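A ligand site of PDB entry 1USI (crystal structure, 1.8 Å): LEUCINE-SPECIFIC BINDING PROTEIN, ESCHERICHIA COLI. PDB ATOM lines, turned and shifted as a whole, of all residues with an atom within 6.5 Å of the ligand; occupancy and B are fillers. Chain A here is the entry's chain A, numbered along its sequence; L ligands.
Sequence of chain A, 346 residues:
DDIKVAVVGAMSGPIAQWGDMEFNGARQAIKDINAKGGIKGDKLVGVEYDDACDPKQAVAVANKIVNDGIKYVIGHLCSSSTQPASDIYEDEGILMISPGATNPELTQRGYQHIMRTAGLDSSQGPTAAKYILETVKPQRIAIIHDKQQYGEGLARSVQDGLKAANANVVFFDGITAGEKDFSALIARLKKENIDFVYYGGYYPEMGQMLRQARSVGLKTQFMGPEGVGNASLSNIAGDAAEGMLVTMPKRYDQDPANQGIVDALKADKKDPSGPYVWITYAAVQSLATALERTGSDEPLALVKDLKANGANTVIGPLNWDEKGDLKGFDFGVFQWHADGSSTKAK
N1 of the ligand lies within salt-bridge range of OE2 of Glu 226, at 2.9 Å.
The side-chain hydroxyl (OH) of Tyr 202 is in hydrogen-bond range of an oxygen (O1) of the ligand (2.7 Å).
The side-chain hydroxyl of Ser 79 sits at hydrogen-bond distance from an oxygen (O2) of the ligand.
An oxygen (O1) of the ligand is in hydrogen-bond range of the backbone NH (N) of Ser 79, 3.0 Å away.
O of Gly 100 lies within hydrogen-bond range of N1 of the ligand, at 2.7 Å.
An oxygen (O2) of the ligand lies within hydrogen-bond range of the backbone NH (N) of Thr 102 (3.0 Å).
A nitrogen (N1) of the ligand lies within hydrogen-bond range of the side-chain hydroxyl of Thr 102, 3.0 Å away.
O of Ala 101 sits at hydrogen-bond distance from NH1 of Arg 116 (2.8 Å).
SG of Cys 53 forms a disulfide with SG of Cys 78.
The backbone NH (N) of Thr 102 sits at hydrogen-bond distance from the side-chain hydroxyl (OG) of Ser 79, at 3.4 Å.
N of Gly 227 lies within hydrogen-bond range of OH of Tyr 150 (3.0 Å).
The backbone NH of Asn 103 lies within hydrogen-bond range of the side-chain hydroxyl of Ser 79.
The side-chain carboxylate (OE2) of Glu 226 is in hydrogen-bond range of the side-chain hydroxyl (OH) of Tyr 276, 2.6 Å away.
The backbone NH of Glu 226 sits at hydrogen-bond distance from the side-chain amide oxygen of Gln 124, at 2.9 Å.
The backbone carbonyl oxygen (O) of Gly 227 sits at hydrogen-bond distance from the indole nitrogen (NE1) of Trp 18.
Merely in contact with the ligand: Trp 18, Leu 77, Cys 78, Ala 101, Tyr 150, Gly 227 and Tyr 276.
Of the 27 residues printed, 12 come within 4 Å of the ligand.
The nearest printed residue that does not touch the ligand is Asn 103 (4.2 Å).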
ATOM      1  N   ILE A  15      -6.243  20.468   3.571  1.00  0.00           N
ATOM      2  CA  ILE A  15      -5.358  19.558   4.301  1.00  0.00           C
ATOM      3  C   ILE A  15      -3.910  20.047   4.404  1.00  0.00           C
ATOM      4  O   ILE A  15      -2.949  19.238   4.461  1.00  0.00           O
ATOM      5  CB  ILE A  15      -5.424  18.111   3.777  1.00  0.00           C
ATOM      6  CG1 ILE A  15      -4.941  18.071   2.313  1.00  0.00           C
ATOM      7  CG2 ILE A  15      -6.875  17.577   4.005  1.00  0.00           C
ATOM      8  CD1 ILE A  15      -4.857  16.625   1.823  1.00  0.00           C
ATOM      9  N   TRP A  18      -1.173  18.513   6.868  1.00  0.00           N
ATOM     10  CA  TRP A  18      -0.320  17.360   6.540  1.00  0.00           C
ATOM     11  C   TRP A  18       0.869  17.885   5.819  1.00  0.00           C
ATOM     12  O   TRP A  18       1.998  17.438   5.996  1.00  0.00           O
ATOM     13  CB  TRP A  18      -1.071  16.381   5.624  1.00  0.00           C
ATOM     14  CG  TRP A  18      -2.014  15.509   6.295  1.00  0.00           C
ATOM     15  CD1 TRP A  18      -3.267  15.236   5.890  1.00  0.00           C
ATOM     16  CD2 TRP A  18      -1.794  14.687   7.473  1.00  0.00           C
ATOM     17  NE1 TRP A  18      -3.877  14.353   6.744  1.00  0.00           N
ATOM     18  CE2 TRP A  18      -2.994  14.010   7.733  1.00  0.00           C
ATOM     19  CE3 TRP A  18      -0.706  14.457   8.324  1.00  0.00           C
ATOM     20  CZ2 TRP A  18      -3.144  13.108   8.778  1.00  0.00           C
ATOM     21  CZ3 TRP A  18      -0.868  13.578   9.394  1.00  0.00           C
ATOM     22  CH2 TRP A  18      -2.061  12.937   9.614  1.00  0.00           C
ATOM     23  N   GLY A  19       0.649  18.876   4.996  1.00  0.00           N
ATOM     24  CA  GLY A  19       1.782  19.542   4.335  1.00  0.00           C
ATOM     25  C   GLY A  19       2.755  20.198   5.285  1.00  0.00           C
ATOM     26  O   GLY A  19       3.948  20.155   5.073  1.00  0.00           O
ATOM     27  N   MET A  21       3.646  19.195   8.156  1.00  0.00           N
ATOM     28  CA  MET A  21       4.534  18.139   8.585  1.00  0.00           C
ATOM     29  C   MET A  21       5.599  17.828   7.571  1.00  0.00           C
ATOM     30  O   MET A  21       6.765  17.613   7.899  1.00  0.00           O
ATOM     31  CB  MET A  21       3.716  16.882   8.887  1.00  0.00           C
ATOM     32  CG  MET A  21       2.872  17.047  10.090  1.00  0.00           C
ATOM     33  SD  MET A  21       1.831  15.618  10.494  1.00  0.00           S
ATOM     34  CE  MET A  21       2.540  14.585   9.972  1.00  0.00           C
ATOM     35  N   CYS A  53      -2.557  20.147  -2.790  1.00  0.00           N
ATOM     36  CA  CYS A  53      -3.084  18.796  -2.891  1.00  0.00           C
ATOM     37  C   CYS A  53      -4.259  18.791  -3.901  1.00  0.00           C
ATOM     38  O   CYS A  53      -5.303  18.155  -3.690  1.00  0.00           O
ATOM     39  CB  CYS A  53      -3.404  18.252  -1.515  1.00  0.00           C
ATOM     40  SG  CYS A  53      -2.096  17.158  -0.810  1.00  0.00           S
ATOM     41  N   LEU A  77       2.257  15.086  -2.112  1.00  0.00           N
ATOM     42  CA  LEU A  77       1.790  14.674  -0.813  1.00  0.00           C
ATOM     43  C   LEU A  77       0.598  13.681  -0.916  1.00  0.00           C
ATOM     44  O   LEU A  77       0.623  12.696  -0.199  1.00  0.00           O
ATOM     45  CB  LEU A  77       1.414  15.884   0.021  1.00  0.00           C
ATOM     46  CG  LEU A  77       0.981  15.637   1.477  1.00  0.00           C
ATOM     47  CD1 LEU A  77       2.137  15.036   2.282  1.00  0.00           C
ATOM     48  CD2 LEU A  77       0.618  16.903   2.067  1.00  0.00           C
ATOM     49  N   CYS A  78      -0.399  14.001  -1.707  1.00  0.00           N
ATOM     50  CA  CYS A  78      -1.681  13.253  -1.825  1.00  0.00           C
ATOM     51  C   CYS A  78      -1.584  12.371  -3.081  1.00  0.00           C
ATOM     52  O   CYS A  78      -0.811  12.645  -4.018  1.00  0.00           O
ATOM     53  CB  CYS A  78      -2.872  14.207  -1.952  1.00  0.00           C
ATOM     54  SG  CYS A  78      -2.900  15.265  -0.400  1.00  0.00           S
ATOM     55  N   SER A  79      -2.357  11.325  -3.103  1.00  0.00           N
ATOM     56  CA  SER A  79      -2.321  10.385  -4.220  1.00  0.00           C
ATOM     57  C   SER A  79      -2.772  11.027  -5.511  1.00  0.00           C
ATOM     58  O   SER A  79      -2.150  10.836  -6.552  1.00  0.00           O
ATOM     59  CB  SER A  79      -3.182   9.136  -3.929  1.00  0.00           C
ATOM     60  OG  SER A  79      -2.517   8.316  -2.973  1.00  0.00           O
ATOM     61  N   SER A  80      -3.881  11.773  -5.489  1.00  0.00           N
ATOM     62  CA  SER A  80      -4.463  12.282  -6.719  1.00  0.00           C
ATOM     63  C   SER A  80      -3.716  13.444  -7.279  1.00  0.00           C
ATOM     64  O   SER A  80      -3.945  13.806  -8.391  1.00  0.00           O
ATOM     65  CB  SER A  80      -5.974  12.565  -6.531  1.00  0.00           C
ATOM     66  OG  SER A  80      -6.192  13.591  -5.626  1.00  0.00           O
ATOM     67  N   PRO A  99       6.713  11.136  -0.209  1.00  0.00           N
ATOM     68  CA  PRO A  99       6.624  10.820   1.206  1.00  0.00           C
ATOM     69  C   PRO A  99       5.215  10.688   1.699  1.00  0.00           C
ATOM     70  O   PRO A  99       5.063  10.443   2.901  1.00  0.00           O
ATOM     71  CB  PRO A  99       7.275  12.027   1.891  1.00  0.00           C
ATOM     72  CG  PRO A  99       6.911  13.178   1.032  1.00  0.00           C
ATOM     73  CD  PRO A  99       6.758  12.605  -0.422  1.00  0.00           C
ATOM     74  N   GLY A 100       4.228  10.832   0.806  1.00  0.00           N
ATOM     75  CA  GLY A 100       2.824  10.932   1.188  1.00  0.00           C
ATOM     76  C   GLY A 100       1.797  10.055   0.504  1.00  0.00           C
ATOM     77  O   GLY A 100       0.821   9.592   1.167  1.00  0.00           O
ATOM     78  N   ALA A 101       2.037   9.754  -0.763  1.00  0.00           N
ATOM     79  CA  ALA A 101       1.041   9.055  -1.562  1.00  0.00           C
ATOM     80  C   ALA A 101       1.021   7.573  -1.258  1.00  0.00           C
ATOM     81  O   ALA A 101       2.089   6.909  -1.324  1.00  0.00           O
ATOM     82  CB  ALA A 101       1.255   9.357  -3.046  1.00  0.00           C
ATOM     83  N   THR A 102      -0.154   7.045  -0.884  1.00  0.00           N
ATOM     84  CA  THR A 102      -0.300   5.649  -0.477  1.00  0.00           C
ATOM     85  C   THR A 102      -1.098   4.793  -1.460  1.00  0.00           C
ATOM     86  O   THR A 102      -1.142   3.591  -1.338  1.00  0.00           O
ATOM     87  CB  THR A 102      -0.901   5.523   0.907  1.00  0.00           C
ATOM     88  OG1 THR A 102      -2.106   6.301   0.973  1.00  0.00           O
ATOM     89  CG2 THR A 102       0.038   6.087   1.999  1.00  0.00           C
ATOM     90  N   ASN A 103      -1.798   5.401  -2.387  1.00  0.00           N
ATOM     91  CA  ASN A 103      -2.659   4.670  -3.293  1.00  0.00           C
ATOM     92  C   ASN A 103      -1.768   3.776  -4.167  1.00  0.00           C
ATOM     93  O   ASN A 103      -0.757   4.255  -4.704  1.00  0.00           O
ATOM     94  CB  ASN A 103      -3.526   5.596  -4.130  1.00  0.00           C
ATOM     95  CG  ASN A 103      -4.418   4.814  -5.068  1.00  0.00           C
ATOM     96  OD1 ASN A 103      -4.051   4.542  -6.200  1.00  0.00           O
ATOM     97  ND2 ASN A 103      -5.589   4.420  -4.564  1.00  0.00           N
ATOM     98  N   ARG A 116       8.558   5.722  -3.368  1.00  0.00           N
ATOM     99  CA  ARG A 116       7.866   6.323  -2.184  1.00  0.00           C
ATOM    100  C   ARG A 116       8.595   5.911  -0.922  1.00  0.00           C
ATOM    101  O   ARG A 116       9.199   4.874  -0.886  1.00  0.00           O
ATOM    102  CB  ARG A 116       6.406   5.903  -1.975  1.00  0.00           C
ATOM    103  CG  ARG A 116       5.753   5.087  -2.916  1.00  0.00           C
ATOM    104  CD  ARG A 116       4.344   4.658  -2.486  1.00  0.00           C
ATOM    105  NE  ARG A 116       3.675   3.929  -3.546  1.00  0.00           N
ATOM    106  CZ  ARG A 116       2.435   4.144  -3.947  1.00  0.00           C
ATOM    107  NH1 ARG A 116       1.669   5.093  -3.364  1.00  0.00           N
ATOM    108  NH2 ARG A 116       1.969   3.396  -4.899  1.00  0.00           N
ATOM    109  N   ALA A 118       6.271   6.580   1.677  1.00  0.00           N
ATOM    110  CA  ALA A 118       5.033   6.222   2.241  1.00  0.00           C
ATOM    111  C   ALA A 118       4.721   4.726   2.007  1.00  0.00           C
ATOM    112  O   ALA A 118       5.298   4.105   1.134  1.00  0.00           O
ATOM    113  CB  ALA A 118       3.942   7.120   1.692  1.00  0.00           C
ATOM    114  N   ASP A 121      -1.814   1.461   0.472  1.00  0.00           N
ATOM    115  CA  ASP A 121      -3.168   1.174   0.914  1.00  0.00           C
ATOM    116  C   ASP A 121      -3.584  -0.263   0.652  1.00  0.00           C
ATOM    117  O   ASP A 121      -4.549  -0.692   1.221  1.00  0.00           O
ATOM    118  CB  ASP A 121      -4.129   2.180   0.312  1.00  0.00           C
ATOM    119  CG  ASP A 121      -3.867   3.567   0.824  1.00  0.00           C
ATOM    120  OD1 ASP A 121      -3.404   3.648   2.000  1.00  0.00           O
ATOM    121  OD2 ASP A 121      -3.981   4.615   0.094  1.00  0.00           O
ATOM    122  N   GLN A 124      -2.689  -0.982   4.032  1.00  0.00           N
ATOM    123  CA  GLN A 124      -3.482  -0.258   5.038  1.00  0.00           C
ATOM    124  C   GLN A 124      -4.946  -0.760   5.090  1.00  0.00           C
ATOM    125  O   GLN A 124      -5.565  -0.900   6.191  1.00  0.00           O
ATOM    126  CB  GLN A 124      -3.459   1.252   4.803  1.00  0.00           C
ATOM    127  CG  GLN A 124      -4.080   2.036   5.970  1.00  0.00           C
ATOM    128  CD  GLN A 124      -3.829   3.519   5.953  1.00  0.00           C
ATOM    129  OE1 GLN A 124      -4.051   4.151   6.978  1.00  0.00           O
ATOM    130  NE2 GLN A 124      -3.477   4.096   4.806  1.00  0.00           N
ATOM    131  N   TYR A 150      -7.638   8.469  -3.107  1.00  0.00           N
ATOM    132  CA  TYR A 150      -7.134   7.951  -1.871  1.00  0.00           C
ATOM    133  C   TYR A 150      -8.280   7.325  -1.053  1.00  0.00           C
ATOM    134  O   TYR A 150      -8.221   6.166  -0.685  1.00  0.00           O
ATOM    135  CB  TYR A 150      -6.447   9.054  -1.082  1.00  0.00           C
ATOM    136  CG  TYR A 150      -6.160   8.720   0.385  1.00  0.00           C
ATOM    137  CD1 TYR A 150      -5.147   7.841   0.746  1.00  0.00           C
ATOM    138  CD2 TYR A 150      -6.901   9.329   1.408  1.00  0.00           C
ATOM    139  CE1 TYR A 150      -4.849   7.569   2.070  1.00  0.00           C
ATOM    140  CE2 TYR A 150      -6.661   9.036   2.710  1.00  0.00           C
ATOM    141  CZ  TYR A 150      -5.620   8.146   3.067  1.00  0.00           C
ATOM    142  OH  TYR A 150      -5.363   7.918   4.392  1.00  0.00           O
ATOM    143  N   GLY A 151      -9.290   8.135  -0.754  1.00  0.00           N
ATOM    144  CA  GLY A 151     -10.317   7.723   0.191  1.00  0.00           C
ATOM    145  C   GLY A 151     -11.211   6.657  -0.346  1.00  0.00           C
ATOM    146  O   GLY A 151     -11.509   5.645   0.318  1.00  0.00           O
ATOM    147  N   TYR A 202     -10.085  12.204   4.665  1.00  0.00           N
ATOM    148  CA  TYR A 202      -9.174  13.035   5.493  1.00  0.00           C
ATOM    149  C   TYR A 202      -9.886  13.682   6.672  1.00  0.00           C
ATOM    150  O   TYR A 202     -11.161  13.717   6.800  1.00  0.00           O
ATOM    151  CB  TYR A 202      -8.529  14.119   4.605  1.00  0.00           C
ATOM    152  CG  TYR A 202      -7.791  13.635   3.387  1.00  0.00           C
ATOM    153  CD1 TYR A 202      -6.523  13.030   3.480  1.00  0.00           C
ATOM    154  CD2 TYR A 202      -8.326  13.753   2.142  1.00  0.00           C
ATOM    155  CE1 TYR A 202      -5.849  12.605   2.375  1.00  0.00           C
ATOM    156  CE2 TYR A 202      -7.660  13.297   1.033  1.00  0.00           C
ATOM    157  CZ  TYR A 202      -6.410  12.752   1.141  1.00  0.00           C
ATOM    158  OH  TYR A 202      -5.775  12.307  -0.023  1.00  0.00           O
ATOM    159  N   GLU A 226      -4.968   6.748   7.772  1.00  0.00           N
ATOM    160  CA  GLU A 226      -4.025   7.657   8.439  1.00  0.00           C
ATOM    161  C   GLU A 226      -4.298   9.136   8.073  1.00  0.00           C
ATOM    162  O   GLU A 226      -3.946  10.050   8.847  1.00  0.00           O
ATOM    163  CB  GLU A 226      -2.609   7.252   8.135  1.00  0.00           C
ATOM    164  CG  GLU A 226      -1.898   8.042   7.079  1.00  0.00           C
ATOM    165  CD  GLU A 226      -2.275   7.697   5.646  1.00  0.00           C
ATOM    166  OE1 GLU A 226      -3.223   6.950   5.385  1.00  0.00           O
ATOM    167  OE2 GLU A 226      -1.514   8.125   4.788  1.00  0.00           O
ATOM    168  N   GLY A 227      -4.951   9.352   6.957  1.00  0.00           N
ATOM    169  CA  GLY A 227      -5.433  10.637   6.541  1.00  0.00           C
ATOM    170  C   GLY A 227      -6.296  11.388   7.543  1.00  0.00           C
ATOM    171  O   GLY A 227      -6.390  12.619   7.481  1.00  0.00           O
ATOM    172  N   VAL A 228      -6.939  10.681   8.477  1.00  0.00           N
ATOM    173  CA  VAL A 228      -7.734  11.324   9.499  1.00  0.00           C
ATOM    174  C   VAL A 228      -7.026  11.567  10.811  1.00  0.00           C
ATOM    175  O   VAL A 228      -7.567  12.265  11.613  1.00  0.00           O
ATOM    176  CB  VAL A 228      -9.035  10.576   9.796  1.00  0.00           C
ATOM    177  CG1 VAL A 228      -9.811  10.412   8.485  1.00  0.00           C
ATOM    178  CG2 VAL A 228      -8.883   9.237  10.532  1.00  0.00           C
ATOM    179  N   ASN A 230      -4.763  13.189  12.748  1.00  0.00           N
ATOM    180  CA  ASN A 230      -4.052  14.483  12.741  1.00  0.00           C
ATOM    181  C   ASN A 230      -4.387  15.141  14.095  1.00  0.00           C
ATOM    182  O   ASN A 230      -5.451  14.893  14.649  1.00  0.00           O
ATOM    183  CB  ASN A 230      -4.743  15.322  11.619  1.00  0.00           C
ATOM    184  CG  ASN A 230      -3.919  16.426  11.088  1.00  0.00           C
ATOM    185  OD1 ASN A 230      -4.359  17.564  11.159  1.00  0.00           O
ATOM    186  ND2 ASN A 230      -2.747  16.150  10.581  1.00  0.00           N
ATOM    187  N   PRO A 275       3.625  11.278  11.941  1.00  0.00           N
ATOM    188  CA  PRO A 275       4.485  10.311  11.243  1.00  0.00           C
ATOM    189  C   PRO A 275       5.125  10.911  10.015  1.00  0.00           C
ATOM    190  O   PRO A 275       6.210  10.445   9.637  1.00  0.00           O
ATOM    191  CB  PRO A 275       3.487   9.218  10.797  1.00  0.00           C
ATOM    192  CG  PRO A 275       2.210   9.875  10.768  1.00  0.00           C
ATOM    193  CD  PRO A 275       2.241  10.785  12.016  1.00  0.00           C
ATOM    194  N   TYR A 276       4.458  11.863   9.370  1.00  0.00           N
ATOM    195  CA  TYR A 276       4.878  12.370   8.053  1.00  0.00           C
ATOM    196  C   TYR A 276       6.033  13.343   8.128  1.00  0.00           C
ATOM    197  O   TYR A 276       6.716  13.546   7.138  1.00  0.00           O
ATOM    198  CB  TYR A 276       3.716  12.900   7.177  1.00  0.00           C
ATOM    199  CG  TYR A 276       2.971  11.701   6.603  1.00  0.00           C
ATOM    200  CD1 TYR A 276       1.915  11.141   7.315  1.00  0.00           C
ATOM    201  CD2 TYR A 276       3.436  11.044   5.464  1.00  0.00           C
ATOM    202  CE1 TYR A 276       1.267   9.958   6.857  1.00  0.00           C
ATOM    203  CE2 TYR A 276       2.800   9.837   4.982  1.00  0.00           C
ATOM    204  CZ  TYR A 276       1.694   9.319   5.643  1.00  0.00           C
ATOM    205  OH  TYR A 276       1.080   8.180   5.117  1.00  0.00           O
HETATM  206  N1  LIG L   1      -1.644   9.036   2.083  1.00  0.00           N
HETATM  207  C1  LIG L   1      -2.556  10.068   1.608  1.00  0.00           C
HETATM  208  C2  LIG L   1      -2.818   9.995   0.114  1.00  0.00           C
HETATM  209  O1  LIG L   1      -3.532  10.870  -0.370  1.00  0.00           O
HETATM  210  C3  LIG L   1      -2.004  11.487   1.899  1.00  0.00           C
HETATM  211  C4  LIG L   1      -1.535  11.701   3.296  1.00  0.00           C
HETATM  212  C5  LIG L   1      -0.336  12.338   3.557  1.00  0.00           C
HETATM  213  C6  LIG L   1      -2.340  11.368   4.370  1.00  0.00           C
HETATM  214  C7  LIG L   1       0.054  12.587   4.871  1.00  0.00           C
HETATM  215  C8  LIG L   1      -1.960  11.591   5.638  1.00  0.00           C
HETATM  216  C9  LIG L   1      -0.764  12.172   5.908  1.00  0.00           C
HETATM  217  O2  LIG L   1      -2.264   9.154  -0.560  1.00  0.00           O
